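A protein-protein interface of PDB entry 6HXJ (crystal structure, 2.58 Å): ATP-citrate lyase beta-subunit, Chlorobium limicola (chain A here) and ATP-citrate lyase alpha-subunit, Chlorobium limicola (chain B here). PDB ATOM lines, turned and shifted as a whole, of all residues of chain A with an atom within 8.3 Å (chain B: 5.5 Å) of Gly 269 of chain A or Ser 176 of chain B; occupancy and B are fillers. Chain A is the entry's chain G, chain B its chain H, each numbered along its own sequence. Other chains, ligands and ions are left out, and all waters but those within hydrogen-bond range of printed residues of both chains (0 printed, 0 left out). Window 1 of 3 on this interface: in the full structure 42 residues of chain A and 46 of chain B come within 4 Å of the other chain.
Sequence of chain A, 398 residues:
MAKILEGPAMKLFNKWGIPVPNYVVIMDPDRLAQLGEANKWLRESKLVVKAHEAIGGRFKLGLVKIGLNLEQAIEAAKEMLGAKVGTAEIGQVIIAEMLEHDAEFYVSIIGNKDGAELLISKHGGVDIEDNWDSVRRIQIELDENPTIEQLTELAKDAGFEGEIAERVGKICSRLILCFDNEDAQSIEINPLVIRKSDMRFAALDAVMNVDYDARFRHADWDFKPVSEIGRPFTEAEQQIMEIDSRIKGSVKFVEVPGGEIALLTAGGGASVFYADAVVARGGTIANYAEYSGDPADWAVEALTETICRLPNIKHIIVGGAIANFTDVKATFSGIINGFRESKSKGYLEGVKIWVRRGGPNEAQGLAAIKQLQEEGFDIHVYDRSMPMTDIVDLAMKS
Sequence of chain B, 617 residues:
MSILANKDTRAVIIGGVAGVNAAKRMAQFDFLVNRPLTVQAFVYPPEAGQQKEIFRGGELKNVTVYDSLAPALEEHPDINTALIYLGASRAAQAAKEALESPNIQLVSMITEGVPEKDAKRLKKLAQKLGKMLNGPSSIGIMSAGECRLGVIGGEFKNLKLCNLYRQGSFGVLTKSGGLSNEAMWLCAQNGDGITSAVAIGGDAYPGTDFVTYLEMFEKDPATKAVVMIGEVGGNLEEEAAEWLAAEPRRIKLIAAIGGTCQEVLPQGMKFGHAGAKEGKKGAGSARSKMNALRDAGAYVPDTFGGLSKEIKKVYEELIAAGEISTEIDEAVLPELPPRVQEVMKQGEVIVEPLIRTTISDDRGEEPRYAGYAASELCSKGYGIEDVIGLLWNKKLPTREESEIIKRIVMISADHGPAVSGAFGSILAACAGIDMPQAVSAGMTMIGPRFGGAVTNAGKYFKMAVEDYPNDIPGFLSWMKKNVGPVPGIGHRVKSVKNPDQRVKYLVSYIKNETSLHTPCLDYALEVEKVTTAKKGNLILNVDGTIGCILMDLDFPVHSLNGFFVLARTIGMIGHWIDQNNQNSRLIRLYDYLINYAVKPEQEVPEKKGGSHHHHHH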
ATOM      1  N   THR A 265      12.579 -32.770  22.059  1.00  0.00           N
ATOM      2  CA  THR A 265      13.081 -31.525  22.613  1.00  0.00           C
ATOM      3  C   THR A 265      14.261 -31.693  23.583  1.00  0.00           C
ATOM      4  O   THR A 265      14.385 -32.708  24.273  1.00  0.00           O
ATOM      5  CB  THR A 265      11.909 -30.766  23.228  1.00  0.00           C
ATOM      6  OG1 THR A 265      11.253 -31.629  24.151  1.00  0.00           O
ATOM      7  CG2 THR A 265      10.898 -30.322  22.172  1.00  0.00           C
ATOM      8  N   ALA A 266      15.128 -30.667  23.610  1.00  0.00           N
ATOM      9  CA  ALA A 266      16.324 -30.608  24.437  1.00  0.00           C
ATOM     10  C   ALA A 266      16.085 -29.930  25.784  1.00  0.00           C
ATOM     11  O   ALA A 266      15.567 -28.810  25.835  1.00  0.00           O
ATOM     12  CB  ALA A 266      17.428 -29.907  23.685  1.00  0.00           C
ATOM     13  N   GLY A 267      16.480 -30.619  26.854  1.00  0.00           N
ATOM     14  CA  GLY A 267      16.325 -30.153  28.227  1.00  0.00           C
ATOM     15  C   GLY A 267      14.943 -30.421  28.796  1.00  0.00           C
ATOM     16  O   GLY A 267      13.938 -30.242  28.105  1.00  0.00           O
ATOM     17  N   GLY A 268      14.901 -30.830  30.059  1.00  0.00           N
ATOM     18  CA  GLY A 268      13.675 -31.116  30.796  1.00  0.00           C
ATOM     19  C   GLY A 268      12.732 -29.935  30.922  1.00  0.00           C
ATOM     20  O   GLY A 268      11.520 -30.090  30.729  1.00  0.00           O
ATOM     21  N   GLY A 269      13.297 -28.766  31.236  1.00  0.00           N
ATOM     22  CA  GLY A 269      12.567 -27.514  31.379  1.00  0.00           C
ATOM     23  C   GLY A 269      11.877 -27.084  30.103  1.00  0.00           C
ATOM     24  O   GLY A 269      10.668 -26.821  30.115  1.00  0.00           O
ATOM     25  N   ALA A 270      12.634 -27.043  28.983  1.00  0.00           N
ATOM     26  CA  ALA A 270      12.093 -26.683  27.674  1.00  0.00           C
ATOM     27  C   ALA A 270      11.076 -27.717  27.194  1.00  0.00           C
ATOM     28  O   ALA A 270      10.046 -27.310  26.665  1.00  0.00           O
ATOM     29  CB  ALA A 270      13.201 -26.526  26.653  1.00  0.00           C
ATOM     30  N   SER A 271      11.336 -29.041  27.401  1.00  0.00           N
ATOM     31  CA  SER A 271      10.435 -30.136  27.014  1.00  0.00           C
ATOM     32  C   SER A 271       9.050 -29.968  27.607  1.00  0.00           C
ATOM     33  O   SER A 271       8.059 -30.103  26.888  1.00  0.00           O
ATOM     34  CB  SER A 271      11.014 -31.485  27.420  1.00  0.00           C
ATOM     35  OG  SER A 271      12.204 -31.755  26.701  1.00  0.00           O
ATOM     36  N   VAL A 272       8.988 -29.622  28.901  1.00  0.00           N
ATOM     37  CA  VAL A 272       7.745 -29.383  29.638  1.00  0.00           C
ATOM     38  C   VAL A 272       6.987 -28.170  29.067  1.00  0.00           C
ATOM     39  O   VAL A 272       5.780 -28.260  28.855  1.00  0.00           O
ATOM     40  CB  VAL A 272       8.015 -29.291  31.160  1.00  0.00           C
ATOM     41  CG1 VAL A 272       6.793 -28.817  31.909  1.00  0.00           C
ATOM     42  CG2 VAL A 272       8.458 -30.638  31.710  1.00  0.00           C
ATOM     43  N   PHE A 273       7.705 -27.074  28.740  1.00  0.00           N
ATOM     44  CA  PHE A 273       7.085 -25.889  28.141  1.00  0.00           C
ATOM     45  C   PHE A 273       6.554 -26.140  26.718  1.00  0.00           C
ATOM     46  O   PHE A 273       5.509 -25.572  26.372  1.00  0.00           O
ATOM     47  CB  PHE A 273       7.992 -24.667  28.217  1.00  0.00           C
ATOM     48  CG  PHE A 273       7.911 -24.017  29.584  1.00  0.00           C
ATOM     49  CD1 PHE A 273       6.778 -23.310  29.973  1.00  0.00           C
ATOM     50  CD2 PHE A 273       8.958 -24.120  30.487  1.00  0.00           C
ATOM     51  CE1 PHE A 273       6.700 -22.712  31.236  1.00  0.00           C
ATOM     52  CE2 PHE A 273       8.854 -23.563  31.766  1.00  0.00           C
ATOM     53  CZ  PHE A 273       7.749 -22.819  32.112  1.00  0.00           C
ATOM     54  N   TYR A 274       7.205 -27.045  25.939  1.00  0.00           N
ATOM     55  CA  TYR A 274       6.741 -27.436  24.602  1.00  0.00           C
ATOM     56  C   TYR A 274       5.447 -28.265  24.670  1.00  0.00           C
ATOM     57  O   TYR A 274       4.532 -28.064  23.857  1.00  0.00           O
ATOM     58  CB  TYR A 274       7.833 -28.187  23.831  1.00  0.00           C
ATOM     59  CG  TYR A 274       8.786 -27.271  23.087  1.00  0.00           C
ATOM     60  CD1 TYR A 274       8.396 -26.630  21.911  1.00  0.00           C
ATOM     61  CD2 TYR A 274      10.089 -27.071  23.540  1.00  0.00           C
ATOM     62  CE1 TYR A 274       9.276 -25.802  21.210  1.00  0.00           C
ATOM     63  CE2 TYR A 274      10.981 -26.250  22.843  1.00  0.00           C
ATOM     64  CZ  TYR A 274      10.569 -25.611  21.679  1.00  0.00           C
ATOM     65  OH  TYR A 274      11.438 -24.794  20.984  1.00  0.00           O
ATOM     66  N   ALA A 275       5.369 -29.183  25.665  1.00  0.00           N
ATOM     67  CA  ALA A 275       4.207 -30.035  25.907  1.00  0.00           C
ATOM     68  C   ALA A 275       3.038 -29.178  26.343  1.00  0.00           C
ATOM     69  O   ALA A 275       1.941 -29.371  25.823  1.00  0.00           O
ATOM     70  CB  ALA A 275       4.523 -31.079  26.970  1.00  0.00           C
ATOM     71  N   ASP A 276       3.277 -28.213  27.264  1.00  0.00           N
ATOM     72  CA  ASP A 276       2.280 -27.261  27.769  1.00  0.00           C
ATOM     73  C   ASP A 276       1.705 -26.457  26.609  1.00  0.00           C
ATOM     74  O   ASP A 276       0.488 -26.289  26.554  1.00  0.00           O
ATOM     75  CB  ASP A 276       2.909 -26.275  28.772  1.00  0.00           C
ATOM     76  CG  ASP A 276       3.135 -26.766  30.189  1.00  0.00           C
ATOM     77  OD1 ASP A 276       3.308 -27.992  30.378  1.00  0.00           O
ATOM     78  OD2 ASP A 276       3.175 -25.919  31.109  1.00  0.00           O
ATOM     79  N   TYR A 288       6.283 -37.661  25.379  1.00  0.00           N
ATOM     80  CA  TYR A 288       7.159 -36.772  26.123  1.00  0.00           C
ATOM     81  C   TYR A 288       8.567 -37.305  25.913  1.00  0.00           C
ATOM     82  O   TYR A 288       8.826 -38.486  26.160  1.00  0.00           O
ATOM     83  CB  TYR A 288       6.849 -36.665  27.633  1.00  0.00           C
ATOM     84  CG  TYR A 288       7.869 -35.790  28.353  1.00  0.00           C
ATOM     85  CD1 TYR A 288       7.770 -34.406  28.323  1.00  0.00           C
ATOM     86  CD2 TYR A 288       8.985 -36.348  28.981  1.00  0.00           C
ATOM     87  CE1 TYR A 288       8.727 -33.596  28.934  1.00  0.00           C
ATOM     88  CE2 TYR A 288       9.967 -35.544  29.569  1.00  0.00           C
ATOM     89  CZ  TYR A 288       9.835 -34.168  29.539  1.00  0.00           C
ATOM     90  OH  TYR A 288      10.769 -33.358  30.141  1.00  0.00           O
ATOM     91  N   GLU A 290      12.969 -35.939  26.177  1.00  0.00           N
ATOM     92  CA  GLU A 290      14.035 -34.975  26.456  1.00  0.00           C
ATOM     93  C   GLU A 290      15.431 -35.569  26.255  1.00  0.00           C
ATOM     94  O   GLU A 290      15.617 -36.773  26.377  1.00  0.00           O
ATOM     95  CB  GLU A 290      13.878 -34.334  27.848  1.00  0.00           C
ATOM     96  CG  GLU A 290      14.010 -35.299  29.009  1.00  0.00           C
ATOM     97  CD  GLU A 290      14.394 -34.701  30.349  1.00  0.00           C
ATOM     98  OE1 GLU A 290      15.611 -34.538  30.602  1.00  0.00           O
ATOM     99  OE2 GLU A 290      13.481 -34.463  31.174  1.00  0.00           O
ATOM    100  N   SER A 292      19.441 -34.076  27.322  1.00  0.00           N
ATOM    101  CA  SER A 292      20.202 -33.002  27.950  1.00  0.00           C
ATOM    102  C   SER A 292      21.570 -33.477  28.428  1.00  0.00           C
ATOM    103  O   SER A 292      21.881 -34.661  28.323  1.00  0.00           O
ATOM    104  CB  SER A 292      19.399 -32.379  29.092  1.00  0.00           C
ATOM    105  OG  SER A 292      19.088 -33.328  30.098  1.00  0.00           O
ATOM    106  N   GLY A 320      14.024 -26.888  21.751  1.00  0.00           N
ATOM    107  CA  GLY A 320      15.053 -26.635  22.733  1.00  0.00           C
ATOM    108  C   GLY A 320      15.245 -25.151  22.920  1.00  0.00           C
ATOM    109  O   GLY A 320      14.883 -24.346  22.053  1.00  0.00           O
ATOM    110  N   ALA A 321      15.806 -24.795  24.079  1.00  0.00           N
ATOM    111  CA  ALA A 321      16.167 -23.433  24.426  1.00  0.00           C
ATOM    112  C   ALA A 321      17.580 -23.205  23.852  1.00  0.00           C
ATOM    113  O   ALA A 321      17.994 -23.902  22.916  1.00  0.00           O
ATOM    114  CB  ALA A 321      16.171 -23.288  25.941  1.00  0.00           C
ATOM    115  N   ASN A 324      23.646 -24.407  27.051  1.00  0.00           N
ATOM    116  CA  ASN A 324      24.760 -23.805  27.779  1.00  0.00           C
ATOM    117  C   ASN A 324      26.035 -24.571  27.458  1.00  0.00           C
ATOM    118  O   ASN A 324      27.093 -23.964  27.412  1.00  0.00           O
ATOM    119  CB  ASN A 324      24.494 -23.792  29.307  1.00  0.00           C
ATOM    120  CG  ASN A 324      23.273 -23.011  29.778  1.00  0.00           C
ATOM    121  OD1 ASN A 324      23.296 -21.773  29.911  1.00  0.00           O
ATOM    122  ND2 ASN A 324      22.194 -23.727  30.092  1.00  0.00           N
ATOM    123  N   MET A 388      10.856 -19.594  21.382  1.00  0.00           N
ATOM    124  CA  MET A 388      11.011 -21.027  21.697  1.00  0.00           C
ATOM    125  C   MET A 388       9.805 -21.962  21.331  1.00  0.00           C
ATOM    126  O   MET A 388       9.947 -22.828  20.452  1.00  0.00           O
ATOM    127  CB  MET A 388      11.339 -21.206  23.201  1.00  0.00           C
ATOM    128  CG  MET A 388      11.918 -22.573  23.528  1.00  0.00           C
ATOM    129  SD  MET A 388      12.347 -22.838  25.266  1.00  0.00           S
ATOM    130  CE  MET A 388      10.759 -23.334  25.947  1.00  0.00           C
ATOM    131  N   THR A 389       8.635 -21.766  21.989  1.00  0.00           N
ATOM    132  CA  THR A 389       7.422 -22.586  21.828  1.00  0.00           C
ATOM    133  C   THR A 389       6.492 -22.064  20.706  1.00  0.00           C
ATOM    134  O   THR A 389       5.366 -22.565  20.563  1.00  0.00           O
ATOM    135  CB  THR A 389       6.666 -22.712  23.162  1.00  0.00           C
ATOM    136  OG1 THR A 389       6.480 -21.400  23.698  1.00  0.00           O
ATOM    137  CG2 THR A 389       7.386 -23.603  24.171  1.00  0.00           C
ATOM    138  N   THR B 174      15.479 -19.621  37.646  1.00  0.00           N
ATOM    139  CA  THR B 174      14.898 -20.811  37.036  1.00  0.00           C
ATOM    140  C   THR B 174      15.285 -22.046  37.824  1.00  0.00           C
ATOM    141  O   THR B 174      16.255 -22.013  38.572  1.00  0.00           O
ATOM    142  CB  THR B 174      15.346 -20.983  35.575  1.00  0.00           C
ATOM    143  OG1 THR B 174      16.744 -21.268  35.552  1.00  0.00           O
ATOM    144  CG2 THR B 174      15.020 -19.781  34.695  1.00  0.00           C
ATOM    145  N   LYS B 175      14.544 -23.141  37.639  1.00  0.00           N
ATOM    146  CA  LYS B 175      14.892 -24.436  38.211  1.00  0.00           C
ATOM    147  C   LYS B 175      15.819 -25.083  37.143  1.00  0.00           C
ATOM    148  O   LYS B 175      16.969 -25.446  37.434  1.00  0.00           O
ATOM    149  CB  LYS B 175      13.637 -25.273  38.473  1.00  0.00           C
ATOM    150  CG  LYS B 175      12.888 -24.858  39.728  1.00  0.00           C
ATOM    151  CD  LYS B 175      11.624 -25.700  39.922  1.00  0.00           C
ATOM    152  CE  LYS B 175      10.989 -25.582  41.301  1.00  0.00           C
ATOM    153  NZ  LYS B 175       9.690 -26.332  41.399  1.00  0.00           N
ATOM    154  N   SER B 176      15.339 -25.077  35.880  1.00  0.00           N
ATOM    155  CA  SER B 176      15.959 -25.586  34.657  1.00  0.00           C
ATOM    156  C   SER B 176      17.176 -24.764  34.200  1.00  0.00           C
ATOM    157  O   SER B 176      17.105 -23.533  34.115  1.00  0.00           O
ATOM    158  CB  SER B 176      14.918 -25.614  33.538  1.00  0.00           C
ATOM    159  OG  SER B 176      15.444 -25.902  32.250  1.00  0.00           O
ATOM    160  N   GLY B 177      18.248 -25.477  33.847  1.00  0.00           N
ATOM    161  CA  GLY B 177      19.482 -24.900  33.345  1.00  0.00           C
ATOM    162  C   GLY B 177      19.337 -24.308  31.956  1.00  0.00           C
ATOM    163  O   GLY B 177      19.686 -23.142  31.742  1.00  0.00           O
ATOM    164  N   GLY B 178      18.813 -25.105  31.021  1.00  0.00           N
ATOM    165  CA  GLY B 178      18.587 -24.687  29.637  1.00  0.00           C
ATOM    166  C   GLY B 178      17.679 -23.478  29.508  1.00  0.00           C
ATOM    167  O   GLY B 178      17.874 -22.656  28.614  1.00  0.00           O
ATOM    168  N   LEU B 179      16.701 -23.342  30.430  1.00  0.00           N
ATOM    169  CA  LEU B 179      15.746 -22.236  30.438  1.00  0.00           C
ATOM    170  C   LEU B 179      16.277 -20.935  31.019  1.00  0.00           C
ATOM    171  O   LEU B 179      15.649 -19.890  30.803  1.00  0.00           O
ATOM    172  CB  LEU B 179      14.453 -22.618  31.125  1.00  0.00           C
ATOM    173  CG  LEU B 179      13.598 -23.630  30.411  1.00  0.00           C
ATOM    174  CD1 LEU B 179      12.331 -23.837  31.177  1.00  0.00           C
ATOM    175  CD2 LEU B 179      13.303 -23.210  28.977  1.00  0.00           C
ATOM    176  N   SER B 180      17.408 -20.974  31.769  1.00  0.00           N
ATOM    177  CA  SER B 180      17.984 -19.726  32.313  1.00  0.00           C
ATOM    178  C   SER B 180      18.668 -18.956  31.185  1.00  0.00           C
ATOM    179  O   SER B 180      18.576 -17.732  31.147  1.00  0.00           O
ATOM    180  CB  SER B 180      18.892 -19.964  33.520  1.00  0.00           C
ATOM    181  OG  SER B 180      19.916 -20.906  33.250  1.00  0.00           O
ATOM    182  N   ALA B 199      20.233 -20.331  38.360  1.00  0.00           N
ATOM    183  CA  ALA B 199      19.592 -21.614  38.130  1.00  0.00           C
ATOM    184  C   ALA B 199      19.649 -22.248  39.530  1.00  0.00           C
ATOM    185  O   ALA B 199      20.742 -22.437  40.072  1.00  0.00           O
ATOM    186  CB  ALA B 199      20.393 -22.421  37.140  1.00  0.00           C
ATOM    187  N   GLY B 201      18.414 -25.149  40.437  1.00  0.00           N
ATOM    188  CA  GLY B 201      18.520 -26.599  40.347  1.00  0.00           C
ATOM    189  C   GLY B 201      17.160 -27.228  40.223  1.00  0.00           C
ATOM    190  O   GLY B 201      16.164 -26.628  40.635  1.00  0.00           O
ATOM    191  N   GLY B 202      17.112 -28.412  39.625  1.00  0.00           N
ATOM    192  CA  GLY B 202      15.857 -29.131  39.409  1.00  0.00           C
ATOM    193  C   GLY B 202      15.556 -30.225  40.414  1.00  0.00           C
ATOM    194  O   GLY B 202      14.566 -30.948  40.260  1.00  0.00           O
ATOM    195  N   ILE B 229      11.064 -18.792  36.337  1.00  0.00           N
ATOM    196  CA  ILE B 229      10.592 -19.925  35.550  1.00  0.00           C
ATOM    197  C   ILE B 229      10.603 -21.185  36.416  1.00  0.00           C
ATOM    198  O   ILE B 229      11.659 -21.771  36.685  1.00  0.00           O
ATOM    199  CB  ILE B 229      11.337 -20.117  34.201  1.00  0.00           C
ATOM    200  CG1 ILE B 229      11.480 -18.799  33.422  1.00  0.00           C
ATOM    201  CG2 ILE B 229      10.638 -21.184  33.378  1.00  0.00           C
ATOM    202  CD1 ILE B 229      12.247 -18.851  32.197  1.00  0.00           C
ATOM    203  N   GLU B 231       8.262 -24.972  37.674  1.00  0.00           N
ATOM    204  CA  GLU B 231       7.666 -26.192  37.153  1.00  0.00           C
ATOM    205  C   GLU B 231       6.818 -26.817  38.235  1.00  0.00           C
ATOM    206  O   GLU B 231       6.987 -26.483  39.410  1.00  0.00           O
ATOM    207  CB  GLU B 231       8.777 -27.179  36.735  1.00  0.00           C
ATOM    208  CG  GLU B 231       8.401 -28.083  35.573  1.00  0.00           C
ATOM    209  CD  GLU B 231       9.016 -29.469  35.614  1.00  0.00           C
ATOM    210  OE1 GLU B 231       8.387 -30.384  36.198  1.00  0.00           O
ATOM    211  OE2 GLU B 231      10.116 -29.647  35.037  1.00  0.00           O
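Printed residues of chain B that touch a printed residue of chain A: Ser 176, Gly 177, Gly 178, Leu 179, Ile 229 and Glu 231. Hydrophobic or aromatic side chains of chain B within 4 Å of the printed part of chain A: Leu 179 and Ile 229. Along chain B the printed residues that touch a printed residue of chain A span positions 176 to 231. Of the 20 printed residues of chain A, 7 touch a printed residue of chain B. Among the printed residues, 10 pairs touch across the chains. Among the printed residues, no Asp or Glu carboxylate lies within 4 Å of a Lys or Arg side-chain nitrogen of the other chain.
Ser 176 of chain B touches Gly 269 of chain A (OG to CA, 3.4 Å). Gly 269 of chain A touches Leu 179 of chain B (C to CD1, 3.5 Å). CG of Leu 179 of chain B touches N of Ala 270 of chain A, at 3.8 Å. Glu 231 of chain B touches Val 272 of chain A. Phe 273 of chain A touches Leu 179 of chain B (CD2 to CD1, 3.5 Å). Ile 229 of chain B touches Phe 273 of chain A (CG2 to CE2, 3.4 Å). Ala 321 of chain A touches Gly 178 of chain B (CB to O, 3.2 Å). Asn 324 of chain A touches Gly 178 of chain B. Leu 179 of chain B touches Met 388 of chain A (CD2 to SD, 3.9 Å).
NZ of Lys 175 of chain B sits at hydrogen-bond distance from O of Glu 231 of chain B, at 3.4 Å. N of Lys 175 of chain B lies within hydrogen-bond range of O of Ile 229 of chain B. The backbone NH (N) of Leu 179 of chain B is in hydrogen-bond range of the side-chain hydroxyl (OG) of Ser 176 of chain B (3.4 Å). The backbone carbonyl oxygen (O) of Ser 176 of chain B is in hydrogen-bond range of the side-chain hydroxyl (OG1) of Thr 174 of chain B (2.7 Å). The backbone carbonyl oxygen of Gly 177 of chain B is in hydrogen-bond range of the side-chain hydroxyl of Ser 180 of chain B (2.7 Å). OH of Tyr 274 of chain A is in hydrogen-bond range of O of Met 388 of chain A, 2.5 Å away.
The side-chain amide nitrogen (ND2) of Asn 324 of chain A sits at hydrogen-bond distance from the backbone carbonyl oxygen (O) of Gly 177 of chain B (3.1 Å).
Gly 269 of chain A touches just these residues of chain B: Ser 176 and Leu 179. Ser 176 of chain B touches just one residue of chain A: Gly 269 (3.4 Å). Gly 177 of chain B touches one residue of chain A. Of the printed residues of chain A, Ile 229 of chain B touches Phe 273 (3.4 Å). Printed residues of chain A within 4 Å of Glu 231 of chain B: Val 272 (3.8 Å). Printed residues of chain B within 4 Å of Asn 324 of chain A: Gly 177 (3.1 Å) and Gly 178 (3.8 Å). Of the printed residues of chain A, Gly 178 of chain B touches Ala 321 and Asn 324. Of the printed residues of chain B, Met 388 of chain A touches Leu 179. Ala 275 of chain A touches none of the printed residues of chain B. The nearest residue of chain B that does not touch Gly 269 of chain A is Glu 231 of chain B (4.9 Å).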
